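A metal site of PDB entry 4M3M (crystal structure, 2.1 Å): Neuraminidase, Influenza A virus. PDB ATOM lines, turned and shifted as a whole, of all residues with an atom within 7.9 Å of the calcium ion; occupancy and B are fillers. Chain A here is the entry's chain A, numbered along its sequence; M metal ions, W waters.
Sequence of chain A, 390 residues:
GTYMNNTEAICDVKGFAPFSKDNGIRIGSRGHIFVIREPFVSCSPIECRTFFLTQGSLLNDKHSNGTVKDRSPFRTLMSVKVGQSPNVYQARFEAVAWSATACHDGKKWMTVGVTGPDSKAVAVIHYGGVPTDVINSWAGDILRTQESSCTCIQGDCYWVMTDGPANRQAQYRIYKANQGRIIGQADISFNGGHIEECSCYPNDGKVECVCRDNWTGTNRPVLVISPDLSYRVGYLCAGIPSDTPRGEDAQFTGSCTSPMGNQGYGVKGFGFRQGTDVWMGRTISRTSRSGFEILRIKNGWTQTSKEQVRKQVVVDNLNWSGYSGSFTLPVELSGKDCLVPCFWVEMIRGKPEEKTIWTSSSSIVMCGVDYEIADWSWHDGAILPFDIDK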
ATOM      1  N   HIS A 194      -4.577 -32.375   3.136  1.00  0.00           N
ATOM      2  CA  HIS A 194      -4.193 -33.319   2.085  1.00  0.00           C
ATOM      3  C   HIS A 194      -2.829 -32.961   1.506  1.00  0.00           C
ATOM      4  O   HIS A 194      -2.606 -31.820   1.111  1.00  0.00           O
ATOM      5  CB  HIS A 194      -5.247 -33.362   0.985  1.00  0.00           C
ATOM      6  CG  HIS A 194      -5.200 -34.593   0.134  1.00  0.00           C
ATOM      7  ND1 HIS A 194      -4.792 -34.586  -1.176  1.00  0.00           N
ATOM      8  CD2 HIS A 194      -5.533 -35.881   0.418  1.00  0.00           C
ATOM      9  CE1 HIS A 194      -4.867 -35.810  -1.670  1.00  0.00           C
ATOM     10  NE2 HIS A 194      -5.311 -36.614  -0.730  1.00  0.00           N
ATOM     11  N   ARG A 212       0.664 -30.171  -2.682  1.00  0.00           N
ATOM     12  CA  ARG A 212      -0.618 -30.081  -3.369  1.00  0.00           C
ATOM     13  C   ARG A 212      -1.743 -30.743  -2.559  1.00  0.00           C
ATOM     14  O   ARG A 212      -1.701 -31.942  -2.275  1.00  0.00           O
ATOM     15  CB  ARG A 212      -0.514 -30.755  -4.748  1.00  0.00           C
ATOM     16  CG  ARG A 212      -1.838 -31.209  -5.373  1.00  0.00           C
ATOM     17  CD  ARG A 212      -1.547 -31.915  -6.690  1.00  0.00           C
ATOM     18  NE  ARG A 212      -2.716 -32.532  -7.330  1.00  0.00           N
ATOM     19  CZ  ARG A 212      -2.665 -33.126  -8.515  1.00  0.00           C
ATOM     20  NH1 ARG A 212      -3.758 -33.673  -9.042  1.00  0.00           N
ATOM     21  NH2 ARG A 212      -1.521 -33.170  -9.186  1.00  0.00           N
ATOM     22  N   ASP A 213      -2.732 -29.943  -2.175  1.00  0.00           N
ATOM     23  CA  ASP A 213      -3.949 -30.484  -1.602  1.00  0.00           C
ATOM     24  C   ASP A 213      -4.848 -30.875  -2.760  1.00  0.00           C
ATOM     25  O   ASP A 213      -5.213 -30.036  -3.592  1.00  0.00           O
ATOM     26  CB  ASP A 213      -4.623 -29.446  -0.702  1.00  0.00           C
ATOM     27  CG  ASP A 213      -5.916 -29.957  -0.059  1.00  0.00           C
ATOM     28  OD1 ASP A 213      -6.058 -29.804   1.165  1.00  0.00           O
ATOM     29  OD2 ASP A 213      -6.802 -30.479  -0.777  1.00  0.00           O
ATOM     30  N   ASN A 214      -5.202 -32.154  -2.822  1.00  0.00           N
ATOM     31  CA  ASN A 214      -6.069 -32.671  -3.882  1.00  0.00           C
ATOM     32  C   ASN A 214      -7.467 -32.972  -3.349  1.00  0.00           C
ATOM     33  O   ASN A 214      -8.249 -33.665  -4.004  1.00  0.00           O
ATOM     34  CB  ASN A 214      -5.441 -33.922  -4.495  1.00  0.00           C
ATOM     35  CG  ASN A 214      -5.643 -33.999  -5.998  1.00  0.00           C
ATOM     36  OD1 ASN A 214      -5.402 -33.024  -6.723  1.00  0.00           O
ATOM     37  ND2 ASN A 214      -6.085 -35.157  -6.482  1.00  0.00           N
ATOM     38  N   TRP A 215      -7.769 -32.462  -2.160  1.00  0.00           N
ATOM     39  CA  TRP A 215      -9.015 -32.758  -1.454  1.00  0.00           C
ATOM     40  C   TRP A 215      -9.966 -31.562  -1.513  1.00  0.00           C
ATOM     41  O   TRP A 215     -10.920 -31.561  -2.296  1.00  0.00           O
ATOM     42  CB  TRP A 215      -8.689 -33.143  -0.005  1.00  0.00           C
ATOM     43  CG  TRP A 215      -9.844 -33.647   0.784  1.00  0.00           C
ATOM     44  CD1 TRP A 215     -11.114 -33.821   0.347  1.00  0.00           C
ATOM     45  CD2 TRP A 215      -9.833 -34.072   2.152  1.00  0.00           C
ATOM     46  NE1 TRP A 215     -11.904 -34.308   1.353  1.00  0.00           N
ATOM     47  CE2 TRP A 215     -11.143 -34.474   2.474  1.00  0.00           C
ATOM     48  CE3 TRP A 215      -8.845 -34.153   3.138  1.00  0.00           C
ATOM     49  CZ2 TRP A 215     -11.495 -34.938   3.752  1.00  0.00           C
ATOM     50  CZ3 TRP A 215      -9.193 -34.621   4.399  1.00  0.00           C
ATOM     51  CH2 TRP A 215     -10.517 -35.007   4.690  1.00  0.00           C
ATOM     52  N   THR A 216      -9.744 -30.550  -0.683  1.00  0.00           N
ATOM     53  CA  THR A 216     -10.614 -29.364  -0.694  1.00  0.00           C
ATOM     54  C   THR A 216      -9.851 -28.045  -0.769  1.00  0.00           C
ATOM     55  O   THR A 216     -10.475 -26.982  -0.708  1.00  0.00           O
ATOM     56  CB  THR A 216     -11.462 -29.280   0.581  1.00  0.00           C
ATOM     57  OG1 THR A 216     -10.616 -28.851   1.660  1.00  0.00           O
ATOM     58  CG2 THR A 216     -12.100 -30.629   0.919  1.00  0.00           C
ATOM     59  N   GLY A 217      -8.536 -28.093  -0.892  1.00  0.00           N
ATOM     60  CA  GLY A 217      -7.724 -26.884  -0.761  1.00  0.00           C
ATOM     61  C   GLY A 217      -7.229 -26.246  -2.049  1.00  0.00           C
ATOM     62  O   GLY A 217      -6.633 -26.929  -2.895  1.00  0.00           O
ATOM     63  N   THR A 218      -7.468 -24.944  -2.185  1.00  0.00           N
ATOM     64  CA  THR A 218      -6.930 -24.172  -3.323  1.00  0.00           C
ATOM     65  C   THR A 218      -5.655 -23.433  -2.931  1.00  0.00           C
ATOM     66  O   THR A 218      -4.949 -22.876  -3.795  1.00  0.00           O
ATOM     67  CB  THR A 218      -7.944 -23.190  -3.922  1.00  0.00           C
ATOM     68  OG1 THR A 218      -8.346 -22.217  -2.942  1.00  0.00           O
ATOM     69  CG2 THR A 218      -9.159 -23.940  -4.428  1.00  0.00           C
ATOM     70  N   ASN A 219      -5.376 -23.419  -1.633  1.00  0.00           N
ATOM     71  CA  ASN A 219      -4.073 -22.987  -1.140  1.00  0.00           C
ATOM     72  C   ASN A 219      -3.205 -24.222  -0.966  1.00  0.00           C
ATOM     73  O   ASN A 219      -3.728 -25.335  -0.914  1.00  0.00           O
ATOM     74  CB  ASN A 219      -4.213 -22.268   0.197  1.00  0.00           C
ATOM     75  CG  ASN A 219      -5.146 -22.998   1.139  1.00  0.00           C
ATOM     76  OD1 ASN A 219      -5.742 -24.006   0.769  1.00  0.00           O
ATOM     77  ND2 ASN A 219      -5.279 -22.482   2.359  1.00  0.00           N
ATOM     78  N   ARG A 220      -1.889 -24.030  -0.870  1.00  0.00           N
ATOM     79  CA  ARG A 220      -0.957 -25.157  -0.801  1.00  0.00           C
ATOM     80  C   ARG A 220      -0.510 -25.479   0.619  1.00  0.00           C
ATOM     81  O   ARG A 220      -0.169 -24.587   1.393  1.00  0.00           O
ATOM     82  CB  ARG A 220       0.278 -24.895  -1.689  1.00  0.00           C
ATOM     83  CG  ARG A 220      -0.044 -24.813  -3.183  1.00  0.00           C
ATOM     84  CD  ARG A 220       1.208 -24.874  -4.041  1.00  0.00           C
ATOM     85  NE  ARG A 220       0.876 -24.797  -5.468  1.00  0.00           N
ATOM     86  CZ  ARG A 220       0.393 -25.827  -6.168  1.00  0.00           C
ATOM     87  NH1 ARG A 220       0.092 -25.673  -7.440  1.00  0.00           N
ATOM     88  NH2 ARG A 220       0.210 -26.997  -5.571  1.00  0.00           N
ATOM     89  N   PRO A 221      -0.519 -26.775   0.967  1.00  0.00           N
ATOM     90  CA  PRO A 221       0.057 -27.193   2.248  1.00  0.00           C
ATOM     91  C   PRO A 221       1.554 -26.889   2.333  1.00  0.00           C
ATOM     92  O   PRO A 221       2.249 -26.940   1.329  1.00  0.00           O
ATOM     93  CB  PRO A 221      -0.185 -28.709   2.280  1.00  0.00           C
ATOM     94  CG  PRO A 221      -0.551 -29.089   0.882  1.00  0.00           C
ATOM     95  CD  PRO A 221      -1.186 -27.881   0.275  1.00  0.00           C
ATOM     96  N   ASP A 243      -3.006 -23.031  -6.125  1.00  0.00           N
ATOM     97  CA  ASP A 243      -3.302 -24.332  -6.758  1.00  0.00           C
ATOM     98  C   ASP A 243      -4.125 -24.117  -8.036  1.00  0.00           C
ATOM     99  O   ASP A 243      -4.491 -22.978  -8.362  1.00  0.00           O
ATOM    100  CB  ASP A 243      -4.035 -25.276  -5.784  1.00  0.00           C
ATOM    101  CG  ASP A 243      -3.899 -26.763  -6.165  1.00  0.00           C
ATOM    102  OD1 ASP A 243      -4.440 -27.618  -5.419  1.00  0.00           O
ATOM    103  OD2 ASP A 243      -3.252 -27.082  -7.184  1.00  0.00           O
ATOM    104  N   THR A 244      -4.389 -25.201  -8.759  1.00  0.00           N
ATOM    105  CA  THR A 244      -5.234 -25.160  -9.949  1.00  0.00           C
ATOM    106  C   THR A 244      -6.054 -26.456 -10.017  1.00  0.00           C
ATOM    107  O   THR A 244      -5.483 -27.550 -10.009  1.00  0.00           O
ATOM    108  CB  THR A 244      -4.409 -24.990 -11.238  1.00  0.00           C
ATOM    109  OG1 THR A 244      -3.640 -23.783 -11.163  1.00  0.00           O
ATOM    110  CG2 THR A 244      -5.320 -24.923 -12.465  1.00  0.00           C
ATOM    111  N   PRO A 245      -7.388 -26.344 -10.096  1.00  0.00           N
ATOM    112  CA  PRO A 245      -8.179 -25.120 -10.162  1.00  0.00           C
ATOM    113  C   PRO A 245      -8.275 -24.377  -8.829  1.00  0.00           C
ATOM    114  O   PRO A 245      -7.959 -24.942  -7.779  1.00  0.00           O
ATOM    115  CB  PRO A 245      -9.573 -25.637 -10.555  1.00  0.00           C
ATOM    116  CG  PRO A 245      -9.635 -26.989  -9.937  1.00  0.00           C
ATOM    117  CD  PRO A 245      -8.243 -27.546 -10.116  1.00  0.00           C
ATOM    118  N   ARG A 246      -8.680 -23.116  -8.896  1.00  0.00           N
ATOM    119  CA  ARG A 246      -8.824 -22.255  -7.730  1.00  0.00           C
ATOM    120  C   ARG A 246      -9.844 -21.182  -8.098  1.00  0.00           C
ATOM    121  O   ARG A 246     -10.241 -21.073  -9.255  1.00  0.00           O
ATOM    122  CB  ARG A 246      -7.494 -21.589  -7.380  1.00  0.00           C
ATOM    123  CG  ARG A 246      -6.868 -20.833  -8.546  1.00  0.00           C
ATOM    124  CD  ARG A 246      -5.742 -19.880  -8.108  1.00  0.00           C
ATOM    125  NE  ARG A 246      -5.249 -19.070  -9.222  1.00  0.00           N
ATOM    126  CZ  ARG A 246      -4.494 -19.545 -10.211  1.00  0.00           C
ATOM    127  NH1 ARG A 246      -4.100 -18.730 -11.188  1.00  0.00           N
ATOM    128  NH2 ARG A 246      -4.131 -20.822 -10.227  1.00  0.00           N
ATOM    129  N   MET A 260      -8.347 -23.678   2.329  1.00  0.00           N
ATOM    130  CA  MET A 260      -9.425 -22.785   1.946  1.00  0.00           C
ATOM    131  C   MET A 260      -9.731 -22.958   0.460  1.00  0.00           C
ATOM    132  O   MET A 260      -8.913 -23.527  -0.282  1.00  0.00           O
ATOM    133  CB  MET A 260      -9.063 -21.336   2.270  1.00  0.00           C
ATOM    134  CG  MET A 260      -8.698 -21.074   3.728  1.00  0.00           C
ATOM    135  SD  MET A 260     -10.150 -20.928   4.810  1.00  0.00           S
ATOM    136  CE  MET A 260     -10.965 -19.530   4.042  1.00  0.00           C
ATOM    137  N   ASN A 262     -12.500 -24.561  -0.979  1.00  0.00           N
ATOM    138  CA  ASN A 262     -13.441 -25.632  -1.284  1.00  0.00           C
ATOM    139  C   ASN A 262     -13.521 -26.034  -2.761  1.00  0.00           C
ATOM    140  O   ASN A 262     -14.544 -25.835  -3.407  1.00  0.00           O
ATOM    141  CB  ASN A 262     -14.851 -25.306  -0.759  1.00  0.00           C
ATOM    142  CG  ASN A 262     -15.675 -26.560  -0.494  1.00  0.00           C
ATOM    143  OD1 ASN A 262     -15.122 -27.646  -0.272  1.00  0.00           O
ATOM    144  ND2 ASN A 262     -16.996 -26.432  -0.532  1.00  0.00           N
ATOM    145  N   GLN A 263     -12.421 -26.580  -3.290  1.00  0.00           N
ATOM    146  CA  GLN A 263     -12.423 -27.174  -4.619  1.00  0.00           C
ATOM    147  C   GLN A 263     -11.550 -28.428  -4.615  1.00  0.00           C
ATOM    148  O   GLN A 263     -10.615 -28.535  -3.827  1.00  0.00           O
ATOM    149  CB  GLN A 263     -11.904 -26.202  -5.684  1.00  0.00           C
ATOM    150  CG  GLN A 263     -12.660 -24.883  -5.797  1.00  0.00           C
ATOM    151  CD  GLN A 263     -12.247 -24.089  -7.013  1.00  0.00           C
ATOM    152  OE1 GLN A 263     -12.024 -22.883  -6.940  1.00  0.00           O
ATOM    153  NE2 GLN A 263     -12.165 -24.765  -8.159  1.00  0.00           N
ATOM    154  N   GLY A 264     -11.871 -29.363  -5.501  1.00  0.00           N
ATOM    155  CA  GLY A 264     -11.108 -30.588  -5.604  1.00  0.00           C
ATOM    156  C   GLY A 264      -9.935 -30.430  -6.557  1.00  0.00           C
ATOM    157  O   GLY A 264      -9.615 -29.320  -6.986  1.00  0.00           O
ATOM    158  N   TYR A 265      -9.295 -31.555  -6.878  1.00  0.00           N
ATOM    159  CA  TYR A 265      -8.201 -31.603  -7.836  1.00  0.00           C
ATOM    160  C   TYR A 265      -7.045 -30.673  -7.454  1.00  0.00           C
ATOM    161  O   TYR A 265      -7.008 -30.116  -6.363  1.00  0.00           O
ATOM    162  CB  TYR A 265      -8.716 -31.304  -9.258  1.00  0.00           C
ATOM    163  CG  TYR A 265      -7.848 -31.895 -10.353  1.00  0.00           C
ATOM    164  CD1 TYR A 265      -7.511 -33.247 -10.361  1.00  0.00           C
ATOM    165  CD2 TYR A 265      -7.359 -31.103 -11.391  1.00  0.00           C
ATOM    166  CE1 TYR A 265      -6.730 -33.787 -11.365  1.00  0.00           C
ATOM    167  CE2 TYR A 265      -6.576 -31.633 -12.385  1.00  0.00           C
ATOM    168  CZ  TYR A 265      -6.258 -32.966 -12.377  1.00  0.00           C
ATOM    169  OH  TYR A 265      -5.471 -33.487 -13.390  1.00  0.00           O
ATOM    170  N   GLY A 266      -6.072 -30.535  -8.349  1.00  0.00           N
ATOM    171  CA  GLY A 266      -4.903 -29.743  -8.057  1.00  0.00           C
ATOM    172  C   GLY A 266      -3.850 -29.919  -9.112  1.00  0.00           C
ATOM    173  O   GLY A 266      -4.072 -30.575 -10.134  1.00  0.00           O
ATOM    174  N   VAL A 267      -2.700 -29.303  -8.888  1.00  0.00           N
ATOM    175  CA  VAL A 267      -1.571 -29.431  -9.771  1.00  0.00           C
ATOM    176  C   VAL A 267      -0.331 -29.286  -8.909  1.00  0.00           C
ATOM    177  O   VAL A 267      -0.325 -28.490  -7.963  1.00  0.00           O
ATOM    178  CB  VAL A 267      -1.608 -28.366 -10.911  1.00  0.00           C
ATOM    179  CG1 VAL A 267      -1.497 -26.938 -10.340  1.00  0.00           C
ATOM    180  CG2 VAL A 267      -0.545 -28.627 -11.949  1.00  0.00           C
HETATM  181 CA    CA M   1      -6.560 -28.527  -4.811  1.00  0.00          CA
HETATM  182  O   HOH W   1      -7.629 -27.388  -6.011  1.00  0.00           O
HETATM  183  O   HOH W   2      -8.490 -29.766  -3.515  1.00  0.00           O
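Water W1 lies within hydrogen-bond range of the backbone carbonyl oxygen of Gly 264 (2.9 Å) and the backbone carbonyl oxygen of Pro 245 (3.0 Å).
The backbone NH (N) of Gly 217 sits at hydrogen-bond distance from the side-chain carboxylate (OD2) of Asp 213 (3.0 Å). The backbone NH of Trp 215 lies within hydrogen-bond range of the side-chain carboxylate of Asp 213. The backbone carbonyl oxygen (O) of Thr 218 is in hydrogen-bond range of the backbone NH (N) of Asp 243. The backbone NH of Val 267 sits at hydrogen-bond distance from the side-chain carboxylate of Asp 243, at 2.9 Å. NH1 of Arg 220 is in salt-bridge range of OD2 of Asp 243 (3.6 Å). The backbone NH (N) of Gly 266 lies within hydrogen-bond range of the side-chain amide oxygen (OD1) of Asn 214, 3.0 Å away. The backbone carbonyl oxygen (O) of Thr 244 sits close to the backbone NH (N) of Gly 266 (3.5 Å). The backbone carbonyl oxygen of Gly 266 is in hydrogen-bond range of the guanidinium group of Arg 212 (3.3 Å).
The calcium ion is bound by water W1 (2.0 Å), O of Tyr 265 (2.3 Å), O of Asp 213 (2.4 Å), OD1 of Asp 243 (2.4 Å), O of Gly 217 (2.5 Å) and water W2 (2.6 Å).
Gly 264 touches the calcium ion. Gly 266 touches the calcium ion (CA to CA, 3.8 Å). Six residues have an atom within 4 Å of the calcium ion: Asp 213, Gly 217, Asp 243, Gly 264, Tyr 265 and Gly 266.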
